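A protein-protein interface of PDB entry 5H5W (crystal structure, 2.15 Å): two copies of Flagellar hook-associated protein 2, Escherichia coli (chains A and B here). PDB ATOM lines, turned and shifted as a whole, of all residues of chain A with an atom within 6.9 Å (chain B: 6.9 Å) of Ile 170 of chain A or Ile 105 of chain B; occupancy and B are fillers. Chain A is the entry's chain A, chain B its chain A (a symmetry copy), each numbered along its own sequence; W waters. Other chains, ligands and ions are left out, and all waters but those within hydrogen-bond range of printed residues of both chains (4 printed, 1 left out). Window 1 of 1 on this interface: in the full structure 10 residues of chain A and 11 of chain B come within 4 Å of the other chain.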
ATOM      1  N   ALA A 161      -4.116  -3.206 -33.927  1.00  0.00           N
ATOM      2  CA  ALA A 161      -5.290  -3.145 -34.786  1.00  0.00           C
ATOM      3  C   ALA A 161      -6.082  -1.928 -34.370  1.00  0.00           C
ATOM      4  O   ALA A 161      -6.157  -1.620 -33.180  1.00  0.00           O
ATOM      5  CB  ALA A 161      -6.131  -4.410 -34.617  1.00  0.00           C
ATOM      6  N   GLN A 162      -6.644  -1.208 -35.343  1.00  0.00           N
ATOM      7  CA  GLN A 162      -7.570  -0.120 -35.063  1.00  0.00           C
ATOM      8  C   GLN A 162      -8.781  -0.233 -35.968  1.00  0.00           C
ATOM      9  O   GLN A 162      -8.640  -0.242 -37.207  1.00  0.00           O
ATOM     10  CB  GLN A 162      -6.896   1.236 -35.282  1.00  0.00           C
ATOM     11  CG  GLN A 162      -5.863   1.572 -34.200  1.00  0.00           C
ATOM     12  CD  GLN A 162      -5.310   2.967 -34.414  1.00  0.00           C
ATOM     13  OE1 GLN A 162      -4.272   3.126 -35.022  1.00  0.00           O
ATOM     14  NE2 GLN A 162      -6.054   3.984 -33.991  1.00  0.00           N
ATOM     15  N   LEU A 163      -9.966  -0.320 -35.379  1.00  0.00           N
ATOM     16  CA  LEU A 163     -11.167  -0.468 -36.181  1.00  0.00           C
ATOM     17  C   LEU A 163     -12.301   0.326 -35.538  1.00  0.00           C
ATOM     18  O   LEU A 163     -12.158   0.789 -34.401  1.00  0.00           O
ATOM     19  CB  LEU A 163     -11.527  -1.967 -36.326  1.00  0.00           C
ATOM     20  CG  LEU A 163     -11.846  -2.819 -35.076  1.00  0.00           C
ATOM     21  CD1 LEU A 163     -12.570  -4.120 -35.429  1.00  0.00           C
ATOM     22  CD2 LEU A 163     -10.641  -3.133 -34.195  1.00  0.00           C
ATOM     23  N   THR A 164     -13.423   0.501 -36.237  1.00  0.00           N
ATOM     24  CA  THR A 164     -14.633   1.023 -35.579  1.00  0.00           C
ATOM     25  C   THR A 164     -15.809   0.079 -35.869  1.00  0.00           C
ATOM     26  O   THR A 164     -15.988  -0.360 -37.011  1.00  0.00           O
ATOM     27  CB  THR A 164     -14.958   2.477 -35.977  1.00  0.00           C
ATOM     28  OG1 THR A 164     -15.489   2.471 -37.289  1.00  0.00           O
ATOM     29  CG2 THR A 164     -13.700   3.325 -36.003  1.00  0.00           C
ATOM     30  N   VAL A 165     -16.551  -0.277 -34.819  1.00  0.00           N
ATOM     31  CA  VAL A 165     -17.675  -1.186 -34.928  1.00  0.00           C
ATOM     32  C   VAL A 165     -18.927  -0.426 -34.461  1.00  0.00           C
ATOM     33  O   VAL A 165     -19.051  -0.033 -33.265  1.00  0.00           O
ATOM     34  CB  VAL A 165     -17.463  -2.487 -34.097  1.00  0.00           C
ATOM     35  CG1 VAL A 165     -18.689  -3.391 -34.194  1.00  0.00           C
ATOM     36  CG2 VAL A 165     -16.223  -3.241 -34.581  1.00  0.00           C
ATOM     37  N   VAL A 168     -18.188   2.660 -32.907  1.00  0.00           N
ATOM     38  CA  VAL A 168     -17.406   2.640 -31.692  1.00  0.00           C
ATOM     39  C   VAL A 168     -15.928   2.313 -31.997  1.00  0.00           C
ATOM     40  O   VAL A 168     -15.602   1.219 -32.520  1.00  0.00           O
ATOM     41  CB  VAL A 168     -18.012   1.671 -30.671  1.00  0.00           C
ATOM     42  CG1 VAL A 168     -17.172   1.624 -29.435  1.00  0.00           C
ATOM     43  CG2 VAL A 168     -19.451   2.100 -30.311  1.00  0.00           C
ATOM     44  N   ALA A 169     -15.037   3.260 -31.679  1.00  0.00           N
ATOM     45  CA  ALA A 169     -13.589   3.062 -31.853  1.00  0.00           C
ATOM     46  C   ALA A 169     -12.971   1.970 -30.974  1.00  0.00           C
ATOM     47  O   ALA A 169     -13.171   1.923 -29.752  1.00  0.00           O
ATOM     48  CB  ALA A 169     -12.827   4.409 -31.696  1.00  0.00           C
ATOM     49  N   ILE A 170     -12.209   1.081 -31.598  1.00  0.00           N
ATOM     50  CA  ILE A 170     -11.639  -0.041 -30.867  1.00  0.00           C
ATOM     51  C   ILE A 170     -10.176  -0.280 -31.217  1.00  0.00           C
ATOM     52  O   ILE A 170      -9.813  -0.344 -32.395  1.00  0.00           O
ATOM     53  CB  ILE A 170     -12.458  -1.354 -31.099  1.00  0.00           C
ATOM     54  CG1 ILE A 170     -13.886  -1.202 -30.533  1.00  0.00           C
ATOM     55  CG2 ILE A 170     -11.775  -2.553 -30.455  1.00  0.00           C
ATOM     56  CD1 ILE A 170     -14.775  -2.378 -30.903  1.00  0.00           C
ATOM     57  N   GLU A 171      -9.341  -0.414 -30.188  1.00  0.00           N
ATOM     58  CA  GLU A 171      -7.928  -0.716 -30.362  1.00  0.00           C
ATOM     59  C   GLU A 171      -7.677  -2.077 -29.793  1.00  0.00           C
ATOM     60  O   GLU A 171      -8.331  -2.481 -28.824  1.00  0.00           O
ATOM     61  CB  GLU A 171      -7.109   0.287 -29.571  1.00  0.00           C
ATOM     62  CG  GLU A 171      -5.652   0.383 -29.936  1.00  0.00           C
ATOM     63  CD  GLU A 171      -4.930   1.488 -29.107  1.00  0.00           C
ATOM     64  OE1 GLU A 171      -5.617   2.095 -28.250  1.00  0.00           O
ATOM     65  OE2 GLU A 171      -3.692   1.728 -29.307  1.00  0.00           O
ATOM     66  N   ASN A 172      -6.729  -2.798 -30.386  1.00  0.00           N
ATOM     67  CA  ASN A 172      -6.439  -4.180 -29.921  1.00  0.00           C
ATOM     68  C   ASN A 172      -5.022  -4.620 -30.308  1.00  0.00           C
ATOM     69  O   ASN A 172      -4.497  -4.220 -31.365  1.00  0.00           O
ATOM     70  CB  ASN A 172      -7.512  -5.179 -30.393  1.00  0.00           C
ATOM     71  CG  ASN A 172      -7.517  -6.485 -29.566  1.00  0.00           C
ATOM     72  OD1 ASN A 172      -6.642  -7.311 -29.718  1.00  0.00           O
ATOM     73  ND2 ASN A 172      -8.488  -6.638 -28.678  1.00  0.00           N
ATOM     74  N   ILE A 177      -9.618 -10.883 -32.555  1.00  0.00           N
ATOM     75  CA  ILE A 177     -10.224 -10.068 -31.518  1.00  0.00           C
ATOM     76  C   ILE A 177     -11.457 -10.760 -30.952  1.00  0.00           C
ATOM     77  O   ILE A 177     -12.529 -10.718 -31.544  1.00  0.00           O
ATOM     78  CB  ILE A 177     -10.605  -8.677 -32.047  1.00  0.00           C
ATOM     79  CG1 ILE A 177      -9.356  -7.978 -32.627  1.00  0.00           C
ATOM     80  CG2 ILE A 177     -11.321  -7.897 -30.959  1.00  0.00           C
ATOM     81  CD1 ILE A 177      -9.557  -6.568 -33.243  1.00  0.00           C
ATOM     82  N   ASP A 179     -12.080 -10.320 -27.445  1.00  0.00           N
ATOM     83  CA  ASP A 179     -12.213  -9.705 -26.124  1.00  0.00           C
ATOM     84  C   ASP A 179     -12.877  -8.305 -26.213  1.00  0.00           C
ATOM     85  O   ASP A 179     -13.233  -7.715 -25.195  1.00  0.00           O
ATOM     86  CB  ASP A 179     -10.848  -9.676 -25.368  1.00  0.00           C
ATOM     87  CG  ASP A 179      -9.785  -8.762 -26.048  1.00  0.00           C
ATOM     88  OD1 ASP A 179      -9.911  -8.446 -27.240  1.00  0.00           O
ATOM     89  OD2 ASP A 179      -8.797  -8.376 -25.391  1.00  0.00           O
ATOM     90  N   ALA A 180     -13.090  -7.819 -27.431  1.00  0.00           N
ATOM     91  CA  ALA A 180     -13.678  -6.508 -27.653  1.00  0.00           C
ATOM     92  C   ALA A 180     -15.215  -6.518 -27.604  1.00  0.00           C
ATOM     93  O   ALA A 180     -15.817  -5.764 -26.840  1.00  0.00           O
ATOM     94  CB  ALA A 180     -13.165  -5.904 -28.988  1.00  0.00           C
ATOM     95  N   LEU A 181     -15.818  -7.390 -28.415  1.00  0.00           N
ATOM     96  CA  LEU A 181     -17.267  -7.521 -28.552  1.00  0.00           C
ATOM     97  C   LEU A 181     -17.762  -8.794 -27.891  1.00  0.00           C
ATOM     98  O   LEU A 181     -17.184  -9.871 -28.092  1.00  0.00           O
ATOM     99  CB  LEU A 181     -17.645  -7.564 -30.031  1.00  0.00           C
ATOM    100  CG  LEU A 181     -17.041  -6.480 -30.939  1.00  0.00           C
ATOM    101  CD1 LEU A 181     -17.277  -6.846 -32.398  1.00  0.00           C
ATOM    102  CD2 LEU A 181     -17.598  -5.062 -30.623  1.00  0.00           C
ATOM    103  N   GLU A 182     -18.846  -8.677 -27.133  1.00  0.00           N
ATOM    104  CA  GLU A 182     -19.403  -9.820 -26.407  1.00  0.00           C
ATOM    105  C   GLU A 182     -19.745 -10.965 -27.365  1.00  0.00           C
ATOM    106  O   GLU A 182     -20.492 -10.762 -28.331  1.00  0.00           O
ATOM    107  CB  GLU A 182     -20.674  -9.405 -25.648  1.00  0.00           C
ATOM    108  CG  GLU A 182     -20.423  -8.666 -24.345  1.00  0.00           C
ATOM    109  CD  GLU A 182     -21.698  -8.156 -23.659  1.00  0.00           C
ATOM    110  OE1 GLU A 182     -22.826  -8.485 -24.098  1.00  0.00           O
ATOM    111  OE2 GLU A 182     -21.564  -7.421 -22.657  1.00  0.00           O
ATOM    112  N   LEU A 186     -13.632 -11.547 -33.949  1.00  0.00           N
ATOM    113  CA  LEU A 186     -13.399 -10.824 -35.194  1.00  0.00           C
ATOM    114  C   LEU A 186     -11.979 -11.187 -35.675  1.00  0.00           C
ATOM    115  O   LEU A 186     -11.032 -11.114 -34.900  1.00  0.00           O
ATOM    116  CB  LEU A 186     -13.573  -9.344 -34.916  1.00  0.00           C
ATOM    117  CG  LEU A 186     -13.726  -8.281 -36.013  1.00  0.00           C
ATOM    118  CD1 LEU A 186     -14.301  -8.805 -37.346  1.00  0.00           C
ATOM    119  CD2 LEU A 186     -14.561  -7.117 -35.485  1.00  0.00           C
ATOM    120  N   THR B  43     -28.526   2.897 -31.108  1.00  0.00           N
ATOM    121  CA  THR B  43     -27.542   2.451 -30.123  1.00  0.00           C
ATOM    122  C   THR B  43     -26.970   3.672 -29.432  1.00  0.00           C
ATOM    123  O   THR B  43     -26.543   4.644 -30.086  1.00  0.00           O
ATOM    124  CB  THR B  43     -26.422   1.618 -30.740  1.00  0.00           C
ATOM    125  OG1 THR B  43     -26.968   0.399 -31.217  1.00  0.00           O
ATOM    126  CG2 THR B  43     -25.348   1.266 -29.706  1.00  0.00           C
ATOM    127  N   THR B  45     -24.062   4.735 -26.619  1.00  0.00           N
ATOM    128  CA  THR B  45     -22.807   4.307 -26.021  1.00  0.00           C
ATOM    129  C   THR B  45     -22.250   5.382 -25.067  1.00  0.00           C
ATOM    130  O   THR B  45     -22.208   6.580 -25.383  1.00  0.00           O
ATOM    131  CB  THR B  45     -21.775   3.946 -27.112  1.00  0.00           C
ATOM    132  OG1 THR B  45     -22.288   2.907 -27.958  1.00  0.00           O
ATOM    133  CG2 THR B  45     -20.447   3.460 -26.495  1.00  0.00           C
ATOM    134  N   THR B  49     -15.324   6.016 -20.401  1.00  0.00           N
ATOM    135  CA  THR B  49     -14.991   4.623 -20.204  1.00  0.00           C
ATOM    136  C   THR B  49     -14.700   4.352 -18.730  1.00  0.00           C
ATOM    137  O   THR B  49     -14.387   5.251 -17.967  1.00  0.00           O
ATOM    138  CB  THR B  49     -13.710   4.274 -20.981  1.00  0.00           C
ATOM    139  OG1 THR B  49     -12.632   5.068 -20.464  1.00  0.00           O
ATOM    140  CG2 THR B  49     -13.866   4.626 -22.468  1.00  0.00           C
ATOM    141  N   LEU B  86     -20.279  -1.685 -14.392  1.00  0.00           N
ATOM    142  CA  LEU B  86     -20.603  -2.028 -15.767  1.00  0.00           C
ATOM    143  C   LEU B  86     -21.275  -3.389 -15.910  1.00  0.00           C
ATOM    144  O   LEU B  86     -22.335  -3.438 -16.518  1.00  0.00           O
ATOM    145  CB  LEU B  86     -19.373  -1.965 -16.644  1.00  0.00           C
ATOM    146  CG  LEU B  86     -18.806  -0.602 -16.970  1.00  0.00           C
ATOM    147  CD1 LEU B  86     -17.875  -0.830 -18.142  1.00  0.00           C
ATOM    148  CD2 LEU B  86     -19.920   0.411 -17.338  1.00  0.00           C
ATOM    149  N   SER B 103     -24.755  -4.190 -23.751  1.00  0.00           N
ATOM    150  CA  SER B 103     -23.530  -4.974 -23.870  1.00  0.00           C
ATOM    151  C   SER B 103     -22.332  -4.122 -23.441  1.00  0.00           C
ATOM    152  O   SER B 103     -22.408  -2.882 -23.427  1.00  0.00           O
ATOM    153  CB  SER B 103     -23.344  -5.424 -25.321  1.00  0.00           C
ATOM    154  OG  SER B 103     -23.187  -4.239 -26.107  1.00  0.00           O
ATOM    155  N   ILE B 104     -21.242  -4.805 -23.096  1.00  0.00           N
ATOM    156  CA  ILE B 104     -19.988  -4.164 -22.781  1.00  0.00           C
ATOM    157  C   ILE B 104     -19.025  -4.241 -23.979  1.00  0.00           C
ATOM    158  O   ILE B 104     -18.938  -5.275 -24.647  1.00  0.00           O
ATOM    159  CB  ILE B 104     -19.375  -4.763 -21.496  1.00  0.00           C
ATOM    160  CG1 ILE B 104     -20.254  -4.383 -20.289  1.00  0.00           C
ATOM    161  CG2 ILE B 104     -17.961  -4.207 -21.270  1.00  0.00           C
ATOM    162  CD1 ILE B 104     -19.883  -5.095 -18.957  1.00  0.00           C
ATOM    163  N   ILE B 105     -18.363  -3.127 -24.292  1.00  0.00           N
ATOM    164  CA  ILE B 105     -17.325  -3.111 -25.331  1.00  0.00           C
ATOM    165  C   ILE B 105     -15.946  -2.818 -24.706  1.00  0.00           C
ATOM    166  O   ILE B 105     -15.739  -1.763 -24.106  1.00  0.00           O
ATOM    167  CB  ILE B 105     -17.629  -2.096 -26.446  1.00  0.00           C
ATOM    168  CG1 ILE B 105     -18.929  -2.457 -27.183  1.00  0.00           C
ATOM    169  CG2 ILE B 105     -16.507  -2.067 -27.493  1.00  0.00           C
ATOM    170  CD1 ILE B 105     -20.115  -1.842 -26.584  1.00  0.00           C
ATOM    171  N   ASN B 106     -15.015  -3.756 -24.823  1.00  0.00           N
ATOM    172  CA  ASN B 106     -13.620  -3.455 -24.477  1.00  0.00           C
ATOM    173  C   ASN B 106     -12.975  -2.671 -25.652  1.00  0.00           C
ATOM    174  O   ASN B 106     -12.678  -3.240 -26.675  1.00  0.00           O
ATOM    175  CB  ASN B 106     -12.911  -4.780 -24.175  1.00  0.00           C
ATOM    176  CG  ASN B 106     -11.451  -4.611 -23.723  1.00  0.00           C
ATOM    177  OD1 ASN B 106     -10.820  -3.577 -23.916  1.00  0.00           O
ATOM    178  ND2 ASN B 106     -10.903  -5.670 -23.150  1.00  0.00           N
ATOM    179  N   VAL B 107     -12.811  -1.358 -25.522  1.00  0.00           N
ATOM    180  CA  VAL B 107     -12.263  -0.550 -26.635  1.00  0.00           C
ATOM    181  C   VAL B 107     -10.720  -0.578 -26.699  1.00  0.00           C
ATOM    182  O   VAL B 107     -10.105   0.143 -27.492  1.00  0.00           O
ATOM    183  CB  VAL B 107     -12.781   0.916 -26.613  1.00  0.00           C
ATOM    184  CG1 VAL B 107     -14.316   0.964 -26.770  1.00  0.00           C
ATOM    185  CG2 VAL B 107     -12.335   1.639 -25.353  1.00  0.00           C
ATOM    186  N   GLY B 108     -10.104  -1.407 -25.861  1.00  0.00           N
ATOM    187  CA  GLY B 108      -8.661  -1.470 -25.766  1.00  0.00           C
ATOM    188  C   GLY B 108      -8.108  -0.474 -24.776  1.00  0.00           C
ATOM    189  O   GLY B 108      -8.865   0.262 -24.162  1.00  0.00           O
ATOM    190  N   GLU B 111      -9.787  -0.070 -21.279  1.00  0.00           N
ATOM    191  CA  GLU B 111     -10.993   0.741 -21.123  1.00  0.00           C
ATOM    192  C   GLU B 111     -12.209   0.035 -21.687  1.00  0.00           C
ATOM    193  O   GLU B 111     -12.124  -0.652 -22.709  1.00  0.00           O
ATOM    194  CB  GLU B 111     -10.888   2.123 -21.815  1.00  0.00           C
ATOM    195  CG  GLU B 111      -9.713   3.017 -21.436  1.00  0.00           C
ATOM    196  CD  GLU B 111      -9.617   4.269 -22.362  1.00  0.00           C
ATOM    197  OE1 GLU B 111     -10.185   5.332 -21.996  1.00  0.00           O
ATOM    198  OE2 GLU B 111      -9.003   4.202 -23.471  1.00  0.00           O
ATOM    199  N   TYR B 112     -13.341   0.264 -21.023  1.00  0.00           N
ATOM    200  CA  TYR B 112     -14.612  -0.360 -21.338  1.00  0.00           C
ATOM    201  C   TYR B 112     -15.700   0.675 -21.482  1.00  0.00           C
ATOM    202  O   TYR B 112     -15.792   1.608 -20.689  1.00  0.00           O
ATOM    203  CB  TYR B 112     -15.015  -1.339 -20.231  1.00  0.00           C
ATOM    204  CG  TYR B 112     -13.980  -2.411 -19.991  1.00  0.00           C
ATOM    205  CD1 TYR B 112     -14.096  -3.664 -20.605  1.00  0.00           C
ATOM    206  CD2 TYR B 112     -12.894  -2.170 -19.169  1.00  0.00           C
ATOM    207  CE1 TYR B 112     -13.140  -4.668 -20.400  1.00  0.00           C
ATOM    208  CE2 TYR B 112     -11.909  -3.162 -18.964  1.00  0.00           C
ATOM    209  CZ  TYR B 112     -12.046  -4.404 -19.582  1.00  0.00           C
ATOM    210  OH  TYR B 112     -11.093  -5.373 -19.388  1.00  0.00           O
ATOM    211  N   ARG B 113     -16.533   0.468 -22.496  1.00  0.00           N
ATOM    212  CA  ARG B 113     -17.736   1.246 -22.722  1.00  0.00           C
ATOM    213  C   ARG B 113     -19.005   0.424 -22.522  1.00  0.00           C
ATOM    214  O   ARG B 113     -19.018  -0.811 -22.701  1.00  0.00           O
ATOM    215  CB  ARG B 113     -17.702   1.817 -24.135  1.00  0.00           C
ATOM    216  CG  ARG B 113     -16.682   2.949 -24.255  1.00  0.00           C
ATOM    217  CD  ARG B 113     -16.980   3.815 -25.463  1.00  0.00           C
ATOM    218  NE  ARG B 113     -15.792   4.509 -25.882  1.00  0.00           N
ATOM    219  CZ  ARG B 113     -15.476   5.755 -25.529  1.00  0.00           C
ATOM    220  NH1 ARG B 113     -16.277   6.427 -24.725  1.00  0.00           N
ATOM    221  NH2 ARG B 113     -14.330   6.309 -25.930  1.00  0.00           N
ATOM    222  N   LEU B 114     -20.065   1.101 -22.120  1.00  0.00           N
ATOM    223  CA  LEU B 114     -21.384   0.468 -22.059  1.00  0.00           C
ATOM    224  C   LEU B 114     -22.238   0.880 -23.260  1.00  0.00           C
ATOM    225  O   LEU B 114     -22.372   2.105 -23.580  1.00  0.00           O
ATOM    226  CB  LEU B 114     -22.114   0.810 -20.755  1.00  0.00           C
ATOM    227  CG  LEU B 114     -23.548   0.281 -20.600  1.00  0.00           C
ATOM    228  CD1 LEU B 114     -23.639  -1.290 -20.384  1.00  0.00           C
ATOM    229  CD2 LEU B 114     -24.261   1.017 -19.482  1.00  0.00           C
ATOM    230  N   SER B 115     -22.812  -0.109 -23.937  1.00  0.00           N
ATOM    231  CA  SER B 115     -23.686   0.207 -25.075  1.00  0.00           C
ATOM    232  C   SER B 115     -25.062  -0.287 -24.782  1.00  0.00           C
ATOM    233  O   SER B 115     -25.207  -1.424 -24.310  1.00  0.00           O
ATOM    234  CB  SER B 115     -23.210  -0.459 -26.378  1.00  0.00           C
ATOM    235  OG  SER B 115     -22.432   0.460 -27.121  1.00  0.00           O
ATOM    236  N   VAL B 116     -26.064   0.552 -25.085  1.00  0.00           N
ATOM    237  CA  VAL B 116     -27.468   0.124 -25.022  1.00  0.00           C
ATOM    238  C   VAL B 116     -28.125   0.292 -26.386  1.00  0.00           C
ATOM    239  O   VAL B 116     -28.104   1.414 -27.009  1.00  0.00           O
ATOM    240  CB  VAL B 116     -28.280   0.923 -23.980  1.00  0.00           C
ATOM    241  CG1 VAL B 116     -29.716   0.359 -23.885  1.00  0.00           C
ATOM    242  CG2 VAL B 116     -27.615   0.854 -22.614  1.00  0.00           C
HETATM  243  O   HOH W   1     -12.552  -7.635 -22.485  1.00  0.00           O
HETATM  244  O   HOH W   2     -10.130  -4.337 -27.623  1.00  0.00           O
HETATM  245  O   HOH W   3     -19.864  -6.255 -26.996  1.00  0.00           O
HETATM  246  O   HOH W   4     -10.268   3.132 -28.468  1.00  0.00           O
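No position is printed for both chains. Of the 14 pairs that touch across the chains among the printed residues, none has its exchanged pair printed and touching as well.
Of the printed residues of chain B, Val 168 of chain A touches Thr 45 and Val 107. Printed residues of chain B within 4 Å of Ile 170 of chain A: Ile 105 (3.8 Å), Asn 106 (3.9 Å) and Val 107 (3.7 Å). Printed residues of chain B within 4 Å of Glu 171 of chain A: Val 107 and Gly 108. Of the printed residues of chain B, Asp 179 of chain A touches Asn 106 (3.1 Å). Ile 105 of chain B touches just these residues of chain A: Ile 170 (3.8 Å) and Ala 180 (3.4 Å). Printed residues of chain A within 4 Å of Asn 106 of chain B: Ile 170 (3.9 Å), Asp 179 (3.1 Å) and Ala 180 (3.0 Å). Printed residues of chain A within 4 Å of Val 107 of chain B: Val 168 (3.96 Å), Ala 169 (3.3 Å), Ile 170 (3.7 Å) and Glu 171 (2.9 Å). Glu 111 of chain B touches none of the printed residues of chain A. The nearest residue of chain B that does not touch Ile 170 of chain A is Gly 108 of chain B (5.0 Å). The nearest residue of chain A that does not touch Ile 105 of chain B is Val 168 of chain A (4.2 Å). The nearest printed residue of chain B that does not touch Ala 169 of chain A is Arg 113 of chain B (5.3 Å).
Among the printed residues, merely in contact across the chains: Val 168 of chain A with Thr 45 of chain B (3.8 Å), Val 168 of chain A with Val 107 of chain B (3.96 Å), Ala 169 of chain A with Val 107 of chain B (3.3 Å), Ile 170 of chain A with Ile 105 of chain B (3.8 Å), Ile 170 of chain A with Asn 106 of chain B (3.9 Å), Ile 170 of chain A with Val 107 of chain B (3.7 Å), Glu 171 of chain A with Gly 108 of chain B (3.2 Å), Asp 179 of chain A with Asn 106 of chain B (3.1 Å), Ala 180 of chain A with Ile 104 of chain B (3.8 Å), Ala 180 of chain A with Ile 105 of chain B (3.4 Å) and Glu 182 of chain A with Ser 103 of chain B (3.3 Å).
OD1 of Asn 106 of chain B is in hydrogen-bond range of N of Gly 108 of chain B (3.0 Å). The backbone NH of Arg 113 of chain B is in hydrogen-bond range of the backbone carbonyl oxygen of Ile 105 of chain B, 2.9 Å away. The backbone carbonyl oxygen of Leu 163 of chain A sits at hydrogen-bond distance from the backbone NH of Ile 170 of chain A (2.8 Å). The side-chain carboxylate of Asp 179 of chain A is in hydrogen-bond range of the side-chain amide nitrogen of Asn 172 of chain A (2.7 Å). OG1 of Thr 45 of chain B sits at hydrogen-bond distance from OG of Ser 115 of chain B (2.6 Å). O of Ser 103 of chain B sits at hydrogen-bond distance from N of Ser 115 of chain B.
O of Ala 180 of chain A is in hydrogen-bond range of N of Asn 106 of chain B. The side-chain carboxylate of Glu 182 of chain A sits at hydrogen-bond distance from the backbone NH of Ile 104 of chain B, 2.7 Å away. O of Val 107 of chain B sits at hydrogen-bond distance from N of Glu 171 of chain A (2.9 Å).
Of the 16 printed residues of chain A, 7 touch a printed residue of chain B. Hydrophobic or aromatic side chains of chain A within 4 Å of the printed part of chain B: Val 168, Ile 170 and Ala 180. Printed residues of chain B that touch a printed residue of chain A: Thr 45, Ser 103, Ile 104, Ile 105, Asn 106, Val 107 and Gly 108. Hydrophobic or aromatic side chains of chain B that line the printed part of chain A: Ile 104, Ile 105 and Val 107.
Water W3 lies within hydrogen-bond range of the backbone NH of Glu 182 of chain A and the backbone carbonyl oxygen of Ile 104 of chain B. Water W1 bridges ND2 of Asn 106 of chain B (2.7 Å) and O of Asp 179 of chain A (2.8 Å). Water W2 lies within hydrogen-bond range of O of Glu 171 of chain A, O of Asn 106 of chain B, ND2 of Asn 172 of chain A and N of Gly 108 of chain B. Water W4 bridges the backbone carbonyl oxygen of Val 107 of chain B (3.1 Å) and the backbone carbonyl oxygen of Ala 169 of chain A (3.4 Å).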
